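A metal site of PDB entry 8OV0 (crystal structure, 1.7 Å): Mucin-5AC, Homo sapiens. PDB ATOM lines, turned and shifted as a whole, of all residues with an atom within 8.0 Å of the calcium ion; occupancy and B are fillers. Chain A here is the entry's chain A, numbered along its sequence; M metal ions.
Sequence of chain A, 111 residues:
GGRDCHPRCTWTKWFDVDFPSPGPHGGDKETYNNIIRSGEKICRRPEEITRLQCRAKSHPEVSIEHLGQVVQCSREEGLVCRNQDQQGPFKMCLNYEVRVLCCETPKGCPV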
ATOM      1  N   PHE A  15      -2.204  15.920  21.266  1.00  0.00           N
ATOM      2  CA  PHE A  15      -2.716  14.978  22.237  1.00  0.00           C
ATOM      3  C   PHE A  15      -1.556  14.276  22.933  1.00  0.00           C
ATOM      4  O   PHE A  15      -0.569  13.890  22.295  1.00  0.00           O
ATOM      5  CB  PHE A  15      -3.586  13.915  21.574  1.00  0.00           C
ATOM      6  CG  PHE A  15      -4.737  14.467  20.787  1.00  0.00           C
ATOM      7  CD1 PHE A  15      -5.855  14.944  21.417  1.00  0.00           C
ATOM      8  CD2 PHE A  15      -4.681  14.483  19.402  1.00  0.00           C
ATOM      9  CE1 PHE A  15      -6.929  15.438  20.673  1.00  0.00           C
ATOM     10  CE2 PHE A  15      -5.724  14.982  18.647  1.00  0.00           C
ATOM     11  CZ  PHE A  15      -6.854  15.460  19.289  1.00  0.00           C
ATOM     12  N   ASP A  16      -1.713  14.058  24.235  1.00  0.00           N
ATOM     13  CA  ASP A  16      -0.682  13.386  25.015  1.00  0.00           C
ATOM     14  C   ASP A  16      -1.433  12.617  26.107  1.00  0.00           C
ATOM     15  O   ASP A  16      -1.607  13.083  27.233  1.00  0.00           O
ATOM     16  CB  ASP A  16       0.316  14.386  25.611  1.00  0.00           C
ATOM     17  CG  ASP A  16       1.457  13.706  26.343  1.00  0.00           C
ATOM     18  OD1 ASP A  16       1.526  12.469  26.364  1.00  0.00           O
ATOM     19  OD2 ASP A  16       2.255  14.425  26.959  1.00  0.00           O
ATOM     20  N   VAL A  17      -1.930  11.434  25.743  1.00  0.00           N
ATOM     21  CA  VAL A  17      -2.805  10.700  26.651  1.00  0.00           C
ATOM     22  C   VAL A  17      -2.088   9.587  27.389  1.00  0.00           C
ATOM     23  O   VAL A  17      -2.669   9.016  28.332  1.00  0.00           O
ATOM     24  CB  VAL A  17      -4.027  10.130  25.912  1.00  0.00           C
ATOM     25  CG1 VAL A  17      -4.850  11.250  25.312  1.00  0.00           C
ATOM     26  CG2 VAL A  17      -3.599   9.085  24.871  1.00  0.00           C
ATOM     27  N   ASP A  18      -0.873   9.224  27.002  1.00  0.00           N
ATOM     28  CA  ASP A  18      -0.149   8.143  27.643  1.00  0.00           C
ATOM     29  C   ASP A  18       1.196   8.718  28.102  1.00  0.00           C
ATOM     30  O   ASP A  18       1.634   9.761  27.619  1.00  0.00           O
ATOM     31  CB  ASP A  18      -0.002   6.937  26.679  1.00  0.00           C
ATOM     32  CG  ASP A  18       0.627   5.720  27.315  1.00  0.00           C
ATOM     33  OD1 ASP A  18       0.553   5.589  28.552  1.00  0.00           O
ATOM     34  OD2 ASP A  18       1.050   4.804  26.555  1.00  0.00           O
ATOM     35  N   PHE A  19       1.801   8.086  29.110  1.00  0.00           N
ATOM     36  CA  PHE A  19       3.092   8.549  29.629  1.00  0.00           C
ATOM     37  C   PHE A  19       3.936   7.301  29.868  1.00  0.00           C
ATOM     38  O   PHE A  19       3.447   6.352  30.516  1.00  0.00           O
ATOM     39  CB  PHE A  19       2.900   9.349  30.917  1.00  0.00           C
ATOM     40  CG  PHE A  19       4.122  10.134  31.327  1.00  0.00           C
ATOM     41  CD1 PHE A  19       4.352  11.391  30.804  1.00  0.00           C
ATOM     42  CD2 PHE A  19       5.009   9.626  32.261  1.00  0.00           C
ATOM     43  CE1 PHE A  19       5.454  12.126  31.187  1.00  0.00           C
ATOM     44  CE2 PHE A  19       6.123  10.356  32.640  1.00  0.00           C
ATOM     45  CZ  PHE A  19       6.336  11.603  32.102  1.00  0.00           C
ATOM     46  N   PRO A  20       5.175   7.255  29.394  1.00  0.00           N
ATOM     47  CA  PRO A  20       5.934   6.007  29.494  1.00  0.00           C
ATOM     48  C   PRO A  20       6.325   5.678  30.926  1.00  0.00           C
ATOM     49  O   PRO A  20       6.621   6.563  31.730  1.00  0.00           O
ATOM     50  CB  PRO A  20       7.160   6.268  28.604  1.00  0.00           C
ATOM     51  CG  PRO A  20       7.357   7.743  28.683  1.00  0.00           C
ATOM     52  CD  PRO A  20       5.951   8.329  28.739  1.00  0.00           C
ATOM     53  N   GLY A  27       6.017   1.776  27.367  1.00  0.00           N
ATOM     54  CA  GLY A  27       6.126   2.549  26.153  1.00  0.00           C
ATOM     55  C   GLY A  27       5.195   3.742  26.221  1.00  0.00           C
ATOM     56  O   GLY A  27       4.727   4.115  27.291  1.00  0.00           O
ATOM     57  N   ASP A  28       4.959   4.330  25.044  1.00  0.00           N
ATOM     58  CA  ASP A  28       4.082   5.491  24.921  1.00  0.00           C
ATOM     59  C   ASP A  28       3.203   5.202  23.710  1.00  0.00           C
ATOM     60  O   ASP A  28       3.715   5.071  22.592  1.00  0.00           O
ATOM     61  CB  ASP A  28       4.873   6.791  24.732  1.00  0.00           C
ATOM     62  CG  ASP A  28       4.054   8.042  25.045  1.00  0.00           C
ATOM     63  OD1 ASP A  28       3.153   7.960  25.897  1.00  0.00           O
ATOM     64  OD2 ASP A  28       4.315   9.113  24.446  1.00  0.00           O
ATOM     65  N   LYS A  29       1.907   5.042  23.936  1.00  0.00           N
ATOM     66  CA  LYS A  29       0.968   4.605  22.891  1.00  0.00           C
ATOM     67  C   LYS A  29      -0.030   5.737  22.662  1.00  0.00           C
ATOM     68  O   LYS A  29      -1.088   5.774  23.284  1.00  0.00           O
ATOM     69  CB  LYS A  29       0.254   3.279  23.286  1.00  0.00           C
ATOM     70  CG  LYS A  29       1.138   2.169  23.863  1.00  0.00           C
ATOM     71  CD  LYS A  29       2.370   1.926  22.984  1.00  0.00           C
ATOM     72  CE  LYS A  29       3.275   0.790  23.512  1.00  0.00           C
ATOM     73  NZ  LYS A  29       2.470  -0.383  23.961  1.00  0.00           N
ATOM     74  N   GLU A  30       0.331   6.674  21.781  1.00  0.00           N
ATOM     75  CA  GLU A  30      -0.552   7.772  21.401  1.00  0.00           C
ATOM     76  C   GLU A  30      -1.330   7.369  20.155  1.00  0.00           C
ATOM     77  O   GLU A  30      -1.233   7.972  19.092  1.00  0.00           O
ATOM     78  CB  GLU A  30       0.237   9.053  21.179  1.00  0.00           C
ATOM     79  CG  GLU A  30       1.040   9.493  22.373  1.00  0.00           C
ATOM     80  CD  GLU A  30       0.190   9.931  23.545  1.00  0.00           C
ATOM     81  OE1 GLU A  30      -0.988  10.338  23.353  1.00  0.00           O
ATOM     82  OE2 GLU A  30       0.707   9.808  24.677  1.00  0.00           O
ATOM     83  N   ARG A  55       5.912  14.328  17.953  1.00  0.00           N
ATOM     84  CA  ARG A  55       7.125  14.940  18.499  1.00  0.00           C
ATOM     85  C   ARG A  55       7.275  14.569  19.966  1.00  0.00           C
ATOM     86  O   ARG A  55       6.326  14.134  20.628  1.00  0.00           O
ATOM     87  CB  ARG A  55       7.123  16.470  18.331  1.00  0.00           C
ATOM     88  CG  ARG A  55       6.124  17.185  19.231  1.00  0.00           C
ATOM     89  CD  ARG A  55       5.979  18.621  18.800  1.00  0.00           C
ATOM     90  NE  ARG A  55       5.061  19.314  19.681  1.00  0.00           N
ATOM     91  CZ  ARG A  55       4.637  20.553  19.479  1.00  0.00           C
ATOM     92  NH1 ARG A  55       5.076  21.264  18.452  1.00  0.00           N
ATOM     93  NH2 ARG A  55       3.778  21.092  20.331  1.00  0.00           N
ATOM     94  N   LYS A  57       7.291  15.440  23.621  1.00  0.00           N
ATOM     95  CA  LYS A  57       6.533  16.469  24.335  1.00  0.00           C
ATOM     96  C   LYS A  57       7.436  17.538  24.941  1.00  0.00           C
ATOM     97  O   LYS A  57       7.151  18.743  24.845  1.00  0.00           O
ATOM     98  CB  LYS A  57       5.663  15.822  25.411  1.00  0.00           C
ATOM     99  CG  LYS A  57       4.834  16.824  26.218  1.00  0.00           C
ATOM    100  CD  LYS A  57       3.510  17.087  25.569  1.00  0.00           C
ATOM    101  CE  LYS A  57       2.616  17.946  26.443  1.00  0.00           C
ATOM    102  NZ  LYS A  57       1.862  17.080  27.385  1.00  0.00           N
ATOM    103  N   LEU A  79       0.895   7.398  17.114  1.00  0.00           N
ATOM    104  CA  LEU A  79       2.284   7.128  17.448  1.00  0.00           C
ATOM    105  C   LEU A  79       2.382   5.941  18.395  1.00  0.00           C
ATOM    106  O   LEU A  79       1.682   5.884  19.411  1.00  0.00           O
ATOM    107  CB  LEU A  79       2.953   8.335  18.113  1.00  0.00           C
ATOM    108  CG  LEU A  79       4.382   8.064  18.624  1.00  0.00           C
ATOM    109  CD1 LEU A  79       5.262   9.251  18.414  1.00  0.00           C
ATOM    110  CD2 LEU A  79       4.415   7.662  20.119  1.00  0.00           C
ATOM    111  N   LEU A  94      10.925   8.011  25.474  1.00  0.00           N
ATOM    112  CA  LEU A  94      10.586   9.335  25.952  1.00  0.00           C
ATOM    113  C   LEU A  94       9.071   9.527  25.814  1.00  0.00           C
ATOM    114  O   LEU A  94       8.352   8.662  25.296  1.00  0.00           O
ATOM    115  CB  LEU A  94      11.344  10.396  25.156  1.00  0.00           C
ATOM    116  CG  LEU A  94      12.861  10.322  25.343  1.00  0.00           C
ATOM    117  CD1 LEU A  94      13.556  11.305  24.434  1.00  0.00           C
ATOM    118  CD2 LEU A  94      13.279  10.523  26.799  1.00  0.00           C
ATOM    119  N   ASN A  95       8.577  10.668  26.313  1.00  0.00           N
ATOM    120  CA  ASN A  95       7.164  11.030  26.232  1.00  0.00           C
ATOM    121  C   ASN A  95       6.862  11.763  24.921  1.00  0.00           C
ATOM    122  O   ASN A  95       7.467  12.803  24.636  1.00  0.00           O
ATOM    123  CB  ASN A  95       6.740  11.934  27.381  1.00  0.00           C
ATOM    124  CG  ASN A  95       5.247  12.120  27.419  1.00  0.00           C
ATOM    125  OD1 ASN A  95       4.495  11.224  27.068  1.00  0.00           O
ATOM    126  ND2 ASN A  95       4.807  13.327  27.744  1.00  0.00           N
ATOM    127  N   TYR A  96       5.908  11.248  24.142  1.00  0.00           N
ATOM    128  CA  TYR A  96       5.540  11.844  22.868  1.00  0.00           C
ATOM    129  C   TYR A  96       4.124  12.399  22.910  1.00  0.00           C
ATOM    130  O   TYR A  96       3.309  12.062  23.780  1.00  0.00           O
ATOM    131  CB  TYR A  96       5.660  10.838  21.716  1.00  0.00           C
ATOM    132  CG  TYR A  96       7.081  10.403  21.545  1.00  0.00           C
ATOM    133  CD1 TYR A  96       7.946  11.142  20.754  1.00  0.00           C
ATOM    134  CD2 TYR A  96       7.574   9.312  22.235  1.00  0.00           C
ATOM    135  CE1 TYR A  96       9.286  10.789  20.643  1.00  0.00           C
ATOM    136  CE2 TYR A  96       8.908   8.943  22.128  1.00  0.00           C
ATOM    137  CZ  TYR A  96       9.753   9.681  21.327  1.00  0.00           C
ATOM    138  OH  TYR A  96      11.083   9.325  21.216  1.00  0.00           O
ATOM    139  N   GLU A  97       3.828  13.246  21.917  1.00  0.00           N
ATOM    140  CA  GLU A  97       2.491  13.779  21.658  1.00  0.00           C
ATOM    141  C   GLU A  97       2.277  13.780  20.153  1.00  0.00           C
ATOM    142  O   GLU A  97       3.226  13.689  19.366  1.00  0.00           O
ATOM    143  CB  GLU A  97       2.323  15.215  22.212  1.00  0.00           C
ATOM    144  CG  GLU A  97       3.283  16.227  21.588  1.00  0.00           C
ATOM    145  CD  GLU A  97       3.162  17.629  22.210  1.00  0.00           C
ATOM    146  OE1 GLU A  97       2.123  17.911  22.856  1.00  0.00           O
ATOM    147  OE2 GLU A  97       4.087  18.456  22.013  1.00  0.00           O
ATOM    148  N   VAL A  98       1.006  13.854  19.730  1.00  0.00           N
ATOM    149  CA  VAL A  98       0.660  13.786  18.314  1.00  0.00           C
ATOM    150  C   VAL A  98      -0.443  14.798  18.021  1.00  0.00           C
ATOM    151  O   VAL A  98      -1.239  15.159  18.889  1.00  0.00           O
ATOM    152  CB  VAL A  98       0.172  12.388  17.850  1.00  0.00           C
ATOM    153  CG1 VAL A  98       1.288  11.360  18.031  1.00  0.00           C
ATOM    154  CG2 VAL A  98      -1.093  11.983  18.567  1.00  0.00           C
HETATM  155 CA    CA M   1       2.661  10.512  25.623  1.00  0.00          CA
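The backbone NH (N) of Lys 57 lies within hydrogen-bond range of the backbone carbonyl oxygen (O) of Asn 95 (2.8 Å).
The side-chain amino group (NZ) of Lys 57 is in salt-bridge range of the side-chain carboxylate (OD2) of Asp 16, 2.7 Å away.
The side-chain carboxylate of Glu 30 lies within hydrogen-bond range of the backbone NH of Val 17.
The backbone NH of Glu 30 sits at hydrogen-bond distance from the backbone carbonyl oxygen of Leu 79 (2.8 Å).
The side-chain carboxylate (OD1) of Asp 28 lies close to the backbone NH (N) of Phe 19 (3.5 Å).
OD2 of Asp 18 sits at hydrogen-bond distance from N of Lys 29 (2.8 Å).
Of the 18 residues printed, 6 come within 4 Å of the calcium ion.
OE2 of Glu 30 is bound to the calcium ion, 2.3 Å away.
The backbone carbonyl oxygen (O) of Asp 18 is bound to the calcium ion (2.4 Å).
The calcium ion is bound by the side-chain carboxylate (OD1) of Asp 16, 2.4 Å away.
OD1 of Asn 95 binds the calcium ion (2.4 Å).
OD2 of Asp 28 binds the calcium ion (2.5 Å).
O of Tyr 96 is bound to the calcium ion (2.5 Å).
The side-chain carboxylate (OD1) of Asp 28 is bound to the calcium ion (2.6 Å).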
